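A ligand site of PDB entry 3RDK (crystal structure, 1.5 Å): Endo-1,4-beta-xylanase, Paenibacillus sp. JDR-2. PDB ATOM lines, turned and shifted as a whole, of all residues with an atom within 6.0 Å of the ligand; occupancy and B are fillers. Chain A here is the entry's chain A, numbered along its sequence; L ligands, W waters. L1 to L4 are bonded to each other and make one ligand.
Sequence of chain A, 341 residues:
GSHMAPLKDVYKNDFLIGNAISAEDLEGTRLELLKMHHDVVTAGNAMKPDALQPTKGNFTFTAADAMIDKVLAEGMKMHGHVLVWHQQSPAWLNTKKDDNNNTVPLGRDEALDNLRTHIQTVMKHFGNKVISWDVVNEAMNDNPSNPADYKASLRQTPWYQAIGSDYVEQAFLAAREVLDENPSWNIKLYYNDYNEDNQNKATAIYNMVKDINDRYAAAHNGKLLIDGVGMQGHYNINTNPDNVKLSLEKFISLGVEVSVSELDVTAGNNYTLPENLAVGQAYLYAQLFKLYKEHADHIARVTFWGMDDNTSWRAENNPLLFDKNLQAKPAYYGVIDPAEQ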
ATOM      1  N   ALA A  43      13.801 -27.369  -5.670  1.00  0.00           N
ATOM      2  CA  ALA A  43      13.951 -28.323  -6.829  1.00  0.00           C
ATOM      3  C   ALA A  43      14.648 -27.556  -7.994  1.00  0.00           C
ATOM      4  O   ALA A  43      14.100 -26.515  -8.442  1.00  0.00           O
ATOM      5  CB  ALA A  43      12.648 -28.899  -7.283  1.00  0.00           C
ATOM      6  N   GLY A  44      15.805 -28.063  -8.534  1.00  0.00           N
ATOM      7  CA  GLY A  44      16.438 -27.361  -9.639  1.00  0.00           C
ATOM      8  C   GLY A  44      15.519 -27.323 -10.881  1.00  0.00           C
ATOM      9  O   GLY A  44      15.551 -26.318 -11.617  1.00  0.00           O
ATOM     10  N   ASN A  45      14.771 -28.417 -11.087  1.00  0.00           N
ATOM     11  CA  ASN A  45      13.868 -28.497 -12.273  1.00  0.00           C
ATOM     12  C   ASN A  45      12.505 -29.150 -12.024  1.00  0.00           C
ATOM     13  O   ASN A  45      11.601 -28.940 -12.925  1.00  0.00           O
ATOM     14  CB  ASN A  45      14.628 -29.308 -13.409  1.00  0.00           C
ATOM     15  CG  ASN A  45      15.796 -28.559 -13.902  1.00  0.00           C
ATOM     16  OD1 ASN A  45      15.642 -27.493 -14.546  1.00  0.00           O
ATOM     17  ND2 ASN A  45      17.020 -29.078 -13.663  1.00  0.00           N
ATOM     18  N   LYS A  48       9.090 -27.007 -12.116  1.00  0.00           N
ATOM     19  CA  LYS A  48       8.830 -26.009 -13.163  1.00  0.00           C
ATOM     20  C   LYS A  48       7.574 -26.325 -14.000  1.00  0.00           C
ATOM     21  O   LYS A  48       7.058 -27.435 -13.908  1.00  0.00           O
ATOM     22  CB  LYS A  48      10.046 -25.850 -14.089  1.00  0.00           C
ATOM     23  CG  LYS A  48      11.206 -25.177 -13.364  1.00  0.00           C
ATOM     24  CD  LYS A  48      12.513 -25.308 -14.089  1.00  0.00           C
ATOM     25  CE  LYS A  48      13.569 -24.551 -13.294  1.00  0.00           C
ATOM     26  NZ  LYS A  48      14.994 -24.689 -13.866  1.00  0.00           N
ATOM     27  N   HIS A  81       9.617 -23.940  -6.601  1.00  0.00           N
ATOM     28  CA  HIS A  81      10.143 -23.128  -7.703  1.00  0.00           C
ATOM     29  C   HIS A  81       9.702 -23.875  -8.988  1.00  0.00           C
ATOM     30  O   HIS A  81      10.067 -25.021  -9.137  1.00  0.00           O
ATOM     31  CB  HIS A  81      11.699 -23.159  -7.572  1.00  0.00           C
ATOM     32  CG  HIS A  81      12.441 -22.506  -8.706  1.00  0.00           C
ATOM     33  ND1 HIS A  81      12.560 -21.148  -8.757  1.00  0.00           N
ATOM     34  CD2 HIS A  81      13.216 -23.014  -9.703  1.00  0.00           C
ATOM     35  CE1 HIS A  81      13.294 -20.803  -9.819  1.00  0.00           C
ATOM     36  NE2 HIS A  81      13.679 -21.927 -10.443  1.00  0.00           N
ATOM     37  N   VAL A  82       8.900 -23.321  -9.889  1.00  0.00           N
ATOM     38  CA  VAL A  82       8.483 -21.902  -9.971  1.00  0.00           C
ATOM     39  C   VAL A  82       7.192 -21.979 -10.796  1.00  0.00           C
ATOM     40  O   VAL A  82       7.029 -22.810 -11.677  1.00  0.00           O
ATOM     41  CB  VAL A  82       9.563 -21.045 -10.687  1.00  0.00           C
ATOM     42  CG1 VAL A  82      10.047 -21.671 -12.088  1.00  0.00           C
ATOM     43  CG2 VAL A  82       9.109 -19.570 -10.867  1.00  0.00           C
ATOM     44  N   TRP A  85       7.073 -18.755 -15.675  1.00  0.00           N
ATOM     45  CA  TRP A  85       8.356 -18.338 -16.238  1.00  0.00           C
ATOM     46  C   TRP A  85       8.287 -18.433 -17.741  1.00  0.00           C
ATOM     47  O   TRP A  85       7.409 -19.109 -18.240  1.00  0.00           O
ATOM     48  CB  TRP A  85       9.437 -19.347 -15.729  1.00  0.00           C
ATOM     49  CG  TRP A  85      10.889 -18.897 -15.975  1.00  0.00           C
ATOM     50  CD1 TRP A  85      11.416 -17.637 -16.084  1.00  0.00           C
ATOM     51  CD2 TRP A  85      12.008 -19.799 -15.935  1.00  0.00           C
ATOM     52  NE1 TRP A  85      12.780 -17.724 -16.232  1.00  0.00           N
ATOM     53  CE2 TRP A  85      13.156 -19.047 -16.125  1.00  0.00           C
ATOM     54  CE3 TRP A  85      12.100 -21.230 -15.797  1.00  0.00           C
ATOM     55  CZ2 TRP A  85      14.459 -19.625 -16.205  1.00  0.00           C
ATOM     56  CZ3 TRP A  85      13.386 -21.805 -15.891  1.00  0.00           C
ATOM     57  CH2 TRP A  85      14.539 -21.000 -16.087  1.00  0.00           C
ATOM     58  N   GLN A  87      10.861 -19.583 -19.568  1.00  0.00           N
ATOM     59  CA  GLN A  87      11.706 -20.757 -19.987  1.00  0.00           C
ATOM     60  C   GLN A  87      11.072 -22.011 -19.304  1.00  0.00           C
ATOM     61  O   GLN A  87      10.322 -21.910 -18.278  1.00  0.00           O
ATOM     62  CB  GLN A  87      13.174 -20.580 -19.486  1.00  0.00           C
ATOM     63  CG  GLN A  87      13.814 -19.405 -20.155  1.00  0.00           C
ATOM     64  CD  GLN A  87      15.296 -19.268 -19.897  1.00  0.00           C
ATOM     65  OE1 GLN A  87      16.001 -20.205 -19.470  1.00  0.00           O
ATOM     66  NE2 GLN A  87      15.812 -18.080 -20.174  1.00  0.00           N
ATOM     67  N   GLN A  88      11.401 -23.226 -19.790  1.00  0.00           N
ATOM     68  CA  GLN A  88      10.910 -24.464 -19.204  1.00  0.00           C
ATOM     69  C   GLN A  88       9.422 -24.420 -18.909  1.00  0.00           C
ATOM     70  O   GLN A  88       8.918 -24.848 -17.870  1.00  0.00           O
ATOM     71  CB  GLN A  88      11.805 -24.834 -18.027  1.00  0.00           C
ATOM     72  CG  GLN A  88      13.173 -25.245 -18.491  1.00  0.00           C
ATOM     73  CD  GLN A  88      14.070 -25.564 -17.296  1.00  0.00           C
ATOM     74  OE1 GLN A  88      14.797 -24.661 -16.748  1.00  0.00           O
ATOM     75  NE2 GLN A  88      14.122 -26.815 -16.946  1.00  0.00           N
ATOM     76  N   ASN A 137       8.954 -15.631 -12.087  1.00  0.00           N
ATOM     77  CA  ASN A 137      10.402 -15.547 -12.259  1.00  0.00           C
ATOM     78  C   ASN A 137      10.734 -14.706 -13.488  1.00  0.00           C
ATOM     79  O   ASN A 137      10.161 -14.873 -14.533  1.00  0.00           O
ATOM     80  CB  ASN A 137      10.822 -17.059 -12.532  1.00  0.00           C
ATOM     81  CG  ASN A 137      12.251 -17.397 -12.074  1.00  0.00           C
ATOM     82  OD1 ASN A 137      12.781 -16.836 -11.161  1.00  0.00           O
ATOM     83  ND2 ASN A 137      12.904 -18.286 -12.821  1.00  0.00           N
ATOM     84  N   GLU A 138      11.731 -13.853 -13.268  1.00  0.00           N
ATOM     85  CA  GLU A 138      12.499 -13.225 -14.369  1.00  0.00           C
ATOM     86  C   GLU A 138      11.554 -12.477 -15.346  1.00  0.00           C
ATOM     87  O   GLU A 138      11.578 -12.674 -16.597  1.00  0.00           O
ATOM     88  CB  GLU A 138      13.329 -14.304 -15.160  1.00  0.00           C
ATOM     89  CG  GLU A 138      14.355 -14.904 -14.179  1.00  0.00           C
ATOM     90  CD  GLU A 138      15.310 -15.855 -14.852  1.00  0.00           C
ATOM     91  OE1 GLU A 138      15.132 -16.197 -16.067  1.00  0.00           O
ATOM     92  OE2 GLU A 138      16.212 -16.237 -14.129  1.00  0.00           O
ATOM     93  N   ASN A 192      11.089 -13.482  -8.140  1.00  0.00           N
ATOM     94  CA  ASN A 192      12.514 -13.884  -8.172  1.00  0.00           C
ATOM     95  C   ASN A 192      13.140 -13.391  -9.472  1.00  0.00           C
ATOM     96  O   ASN A 192      12.510 -13.492 -10.537  1.00  0.00           O
ATOM     97  CB  ASN A 192      12.504 -15.449  -8.207  1.00  0.00           C
ATOM     98  CG  ASN A 192      13.823 -16.071  -7.898  1.00  0.00           C
ATOM     99  OD1 ASN A 192      14.471 -15.740  -6.915  1.00  0.00           O
ATOM    100  ND2 ASN A 192      14.198 -17.088  -8.739  1.00  0.00           N
ATOM    101  N   TYR A 194      17.216 -12.129 -11.582  1.00  0.00           N
ATOM    102  CA  TYR A 194      18.702 -12.114 -11.553  1.00  0.00           C
ATOM    103  C   TYR A 194      19.198 -10.752 -12.105  1.00  0.00           C
ATOM    104  O   TYR A 194      18.378  -9.962 -12.552  1.00  0.00           O
ATOM    105  CB  TYR A 194      19.317 -13.269 -12.430  1.00  0.00           C
ATOM    106  CG  TYR A 194      19.025 -13.024 -13.889  1.00  0.00           C
ATOM    107  CD1 TYR A 194      17.779 -13.360 -14.380  1.00  0.00           C
ATOM    108  CD2 TYR A 194      19.982 -12.366 -14.763  1.00  0.00           C
ATOM    109  CE1 TYR A 194      17.378 -13.122 -15.736  1.00  0.00           C
ATOM    110  CE2 TYR A 194      19.596 -12.085 -16.142  1.00  0.00           C
ATOM    111  CZ  TYR A 194      18.317 -12.413 -16.582  1.00  0.00           C
ATOM    112  OH  TYR A 194      17.976 -12.154 -17.893  1.00  0.00           O
ATOM    113  N   GLN A 232      18.505 -13.580  -7.129  1.00  0.00           N
ATOM    114  CA  GLN A 232      19.075 -14.920  -7.504  1.00  0.00           C
ATOM    115  C   GLN A 232      20.527 -15.039  -7.154  1.00  0.00           C
ATOM    116  O   GLN A 232      20.993 -16.099  -6.854  1.00  0.00           O
ATOM    117  CB  GLN A 232      18.867 -15.178  -9.003  1.00  0.00           C
ATOM    118  CG  GLN A 232      17.420 -15.574  -9.329  1.00  0.00           C
ATOM    119  CD  GLN A 232      17.183 -15.837 -10.745  1.00  0.00           C
ATOM    120  OE1 GLN A 232      18.171 -16.054 -11.490  1.00  0.00           O
ATOM    121  NE2 GLN A 232      15.904 -15.880 -11.161  1.00  0.00           N
ATOM    122  N   HIS A 234      23.222 -14.916  -9.185  1.00  0.00           N
ATOM    123  CA  HIS A 234      24.081 -15.503 -10.196  1.00  0.00           C
ATOM    124  C   HIS A 234      25.191 -14.495 -10.510  1.00  0.00           C
ATOM    125  O   HIS A 234      25.092 -13.673 -11.469  1.00  0.00           O
ATOM    126  CB  HIS A 234      23.288 -15.896 -11.404  1.00  0.00           C
ATOM    127  CG  HIS A 234      22.432 -17.110 -11.139  1.00  0.00           C
ATOM    128  ND1 HIS A 234      22.981 -18.320 -10.678  1.00  0.00           N
ATOM    129  CD2 HIS A 234      21.106 -17.322 -11.292  1.00  0.00           C
ATOM    130  CE1 HIS A 234      21.988 -19.204 -10.525  1.00  0.00           C
ATOM    131  NE2 HIS A 234      20.851 -18.622 -10.905  1.00  0.00           N
ATOM    132  N   GLU A 262      19.619 -18.272  -5.570  1.00  0.00           N
ATOM    133  CA  GLU A 262      20.330 -19.175  -6.527  1.00  0.00           C
ATOM    134  C   GLU A 262      21.796 -18.763  -6.585  1.00  0.00           C
ATOM    135  O   GLU A 262      22.402 -18.699  -7.706  1.00  0.00           O
ATOM    136  CB  GLU A 262      19.691 -19.051  -7.909  1.00  0.00           C
ATOM    137  CG  GLU A 262      18.179 -19.253  -7.877  1.00  0.00           C
ATOM    138  CD  GLU A 262      17.551 -19.248  -9.324  1.00  0.00           C
ATOM    139  OE1 GLU A 262      18.266 -19.356 -10.387  1.00  0.00           O
ATOM    140  OE2 GLU A 262      16.318 -19.154  -9.391  1.00  0.00           O
ATOM    141  N   TRP A 305      23.131 -22.422  -5.614  1.00  0.00           N
ATOM    142  CA  TRP A 305      22.481 -23.100  -6.705  1.00  0.00           C
ATOM    143  C   TRP A 305      23.360 -24.303  -7.094  1.00  0.00           C
ATOM    144  O   TRP A 305      23.997 -24.357  -8.178  1.00  0.00           O
ATOM    145  CB  TRP A 305      22.312 -22.158  -7.863  1.00  0.00           C
ATOM    146  CG  TRP A 305      21.191 -22.579  -8.785  1.00  0.00           C
ATOM    147  CD1 TRP A 305      21.337 -22.964 -10.119  1.00  0.00           C
ATOM    148  CD2 TRP A 305      19.808 -22.782  -8.424  1.00  0.00           C
ATOM    149  NE1 TRP A 305      20.093 -23.343 -10.630  1.00  0.00           N
ATOM    150  CE2 TRP A 305      19.134 -23.187  -9.636  1.00  0.00           C
ATOM    151  CE3 TRP A 305      19.027 -22.544  -7.268  1.00  0.00           C
ATOM    152  CZ2 TRP A 305      17.770 -23.520  -9.681  1.00  0.00           C
ATOM    153  CZ3 TRP A 305      17.672 -22.807  -7.335  1.00  0.00           C
ATOM    154  CH2 TRP A 305      17.041 -23.318  -8.528  1.00  0.00           C
ATOM    155  N   TRP A 313      24.780 -25.999 -12.956  1.00  0.00           N
ATOM    156  CA  TRP A 313      24.274 -25.660 -14.265  1.00  0.00           C
ATOM    157  C   TRP A 313      25.381 -24.864 -15.058  1.00  0.00           C
ATOM    158  O   TRP A 313      25.220 -24.751 -16.305  1.00  0.00           O
ATOM    159  CB  TRP A 313      22.987 -24.853 -14.132  1.00  0.00           C
ATOM    160  CG  TRP A 313      23.190 -23.425 -13.667  1.00  0.00           C
ATOM    161  CD1 TRP A 313      23.949 -22.961 -12.572  1.00  0.00           C
ATOM    162  CD2 TRP A 313      22.674 -22.215 -14.326  1.00  0.00           C
ATOM    163  NE1 TRP A 313      23.824 -21.554 -12.477  1.00  0.00           N
ATOM    164  CE2 TRP A 313      23.067 -21.110 -13.540  1.00  0.00           C
ATOM    165  CE3 TRP A 313      21.870 -22.011 -15.493  1.00  0.00           C
ATOM    166  CZ2 TRP A 313      22.715 -19.764 -13.899  1.00  0.00           C
ATOM    167  CZ3 TRP A 313      21.502 -20.672 -15.821  1.00  0.00           C
ATOM    168  CH2 TRP A 313      21.932 -19.594 -15.029  1.00  0.00           C
HETATM  169  C1  LIG L   1      17.000 -19.273 -13.610  1.00  0.00           C
HETATM  170  C2  LIG L   1      16.005 -20.240 -12.998  1.00  0.00           C
HETATM  171  C3  LIG L   1      16.657 -21.502 -12.440  1.00  0.00           C
HETATM  172  C4  LIG L   1      17.486 -22.033 -13.643  1.00  0.00           C
HETATM  173  C5  LIG L   1      18.627 -21.110 -13.888  1.00  0.00           C
HETATM  174  O1  LIG L   1      17.835 -18.556 -12.799  1.00  0.00           O
HETATM  175  O2  LIG L   1      15.336 -19.537 -11.957  1.00  0.00           O
HETATM  176  O3  LIG L   1      15.622 -22.465 -12.270  1.00  0.00           O
HETATM  177  O4  LIG L   1      17.990 -23.379 -13.206  1.00  0.00           O
HETATM  178  O5  LIG L   1      17.876 -20.033 -14.595  1.00  0.00           O
HETATM  179  C1  LG2 L   2      18.572 -24.134 -14.253  1.00  0.00           C
HETATM  180  C2  LG2 L   2      18.828 -25.529 -13.762  1.00  0.00           C
HETATM  181  C3  LG2 L   2      19.430 -26.348 -14.871  1.00  0.00           C
HETATM  182  C4  LG2 L   2      18.355 -26.280 -16.001  1.00  0.00           C
HETATM  183  C5  LG2 L   2      18.222 -24.821 -16.504  1.00  0.00           C
HETATM  184  O1  LG2 L   2      19.819 -25.443 -12.747  1.00  0.00           O
HETATM  185  O2  LG2 L   2      19.522 -27.722 -14.488  1.00  0.00           O
HETATM  186  O3  LG2 L   2      18.925 -27.039 -17.256  1.00  0.00           O
HETATM  187  O4  LG2 L   2      17.624 -24.175 -15.316  1.00  0.00           O
HETATM  188  C1  LG3 L   3      17.867 -27.655 -18.083  1.00  0.00           C
HETATM  189  C2  LG3 L   3      18.549 -27.714 -19.472  1.00  0.00           C
HETATM  190  C3  LG3 L   3      17.615 -28.534 -20.247  1.00  0.00           C
HETATM  191  C4  LG3 L   3      17.336 -29.872 -19.403  1.00  0.00           C
HETATM  192  C5  LG3 L   3      16.662 -29.626 -18.032  1.00  0.00           C
HETATM  193  O1  LG3 L   3      19.051 -26.446 -20.020  1.00  0.00           O
HETATM  194  O2  LG3 L   3      18.344 -28.817 -21.508  1.00  0.00           O
HETATM  195  O3  LG3 L   3      16.467 -30.887 -19.971  1.00  0.00           O
HETATM  196  O4  LG3 L   3      17.756 -28.850 -17.371  1.00  0.00           O
HETATM  197  C1  LG4 L   4      22.410 -24.210 -24.248  1.00  0.00           C
HETATM  198  C2  LG4 L   4      20.317 -25.763 -19.894  1.00  0.00           C
HETATM  199  C3  LG4 L   4      20.296 -24.294 -20.309  1.00  0.00           C
HETATM  200  C4  LG4 L   4      19.808 -24.390 -21.754  1.00  0.00           C
HETATM  201  C5  LG4 L   4      21.030 -24.947 -22.493  1.00  0.00           C
HETATM  202  C6  LG4 L   4      20.980 -26.426 -22.108  1.00  0.00           C
HETATM  203  C7  LG4 L   4      22.098 -27.209 -22.844  1.00  0.00           C
HETATM  204  O1  LG4 L   4      19.428 -23.537 -19.464  1.00  0.00           O
HETATM  205  O2  LG4 L   4      19.328 -23.162 -22.308  1.00  0.00           O
HETATM  206  O3  LG4 L   4      21.011 -24.697 -23.891  1.00  0.00           O
HETATM  207  O4  LG4 L   4      21.243 -26.542 -20.722  1.00  0.00           O
HETATM  208  O5  LG4 L   4      22.008 -27.446 -24.067  1.00  0.00           O
HETATM  209  O6  LG4 L   4      23.061 -27.551 -22.156  1.00  0.00           O
HETATM  210  O   HOH W   1      22.869 -25.600 -17.617  1.00  0.00           O
HETATM  211  O   HOH W   2      18.380 -19.325 -17.089  1.00  0.00           O
HETATM  212  O   HOH W   3      19.471 -16.478 -14.561  1.00  0.00           O
HETATM  213  O   HOH W   4      21.957 -28.060 -13.435  1.00  0.00           O
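Residues that only touch the ligand: Gly 44, Trp 85, His 234 and Trp 313.
Within 4 Å of the ligand: Gly 44, Asn 45, Lys 48, His 81, Trp 85, Gln 88, Asn 137, Glu 138, Gln 232, His 234, Glu 262, Trp 305 and Trp 313.
The nearest printed residue that does not touch the ligand is Asn 192 (4.2 Å).
Water W2 bridges O5 of LIG L1 (2.6 Å) and OE1 of Gln 87 (3.5 Å).
Water W3 lies within hydrogen-bond range of an oxygen (O1) of LIG L1, the side-chain carboxylate (OE2) of Glu 138 and the side-chain amide oxygen (OE1) of Gln 232.
O2 of LIG L1 sits at hydrogen-bond distance from ND2 of Asn 137, at 2.9 Å.
The side-chain amide nitrogen (ND2) of Asn 45 lies within hydrogen-bond range of an oxygen (O2) of LG2 L2, 3.0 Å away.
An oxygen (O1) of LIG L1 is in hydrogen-bond range of the side-chain carboxylate (OE2) of Glu 138 (3.1 Å).
O1 of LIG L1 is in hydrogen-bond range of OE1 of Gln 232 (2.8 Å).
O1 of LG2 L2 is in hydrogen-bond range of NE1 of Trp 305, 3.0 Å away.
NE2 of His 81 sits at hydrogen-bond distance from O3 of LIG L1, 2.7 Å away.
The side-chain amide oxygen of Gln 88 sits close to an oxygen (O4) of LG2 L2.
NZ of Lys 48 lies within hydrogen-bond range of O3 of LIG L1.
O1 of LIG L1 is in hydrogen-bond range of OE1 of Glu 262 (2.6 Å).
O of Gly 44 lies within hydrogen-bond range of NZ of Lys 48 (2.8 Å).
ND2 of Asn 192 lies close to NE2 of Gln 232 (3.2 Å).
OD1 of Asn 137 lies within hydrogen-bond range of ND2 of Asn 192.
The side-chain amide nitrogen (ND2) of Asn 137 sits close to the indole nitrogen (NE1) of Trp 85 (3.5 Å).
NZ of Lys 48 lies within hydrogen-bond range of OD1 of Asn 45 (3.0 Å).
The side-chain amide nitrogen (NE2) of Gln 232 is in hydrogen-bond range of the side-chain amide oxygen (OD1) of Asn 137 (3.3 Å).
OE2 of Glu 262 sits at hydrogen-bond distance from ND2 of Asn 192 (3.0 Å).
The side-chain amino group (NZ) of Lys 48 sits at hydrogen-bond distance from the side-chain amide oxygen (OE1) of Gln 88 (2.9 Å).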
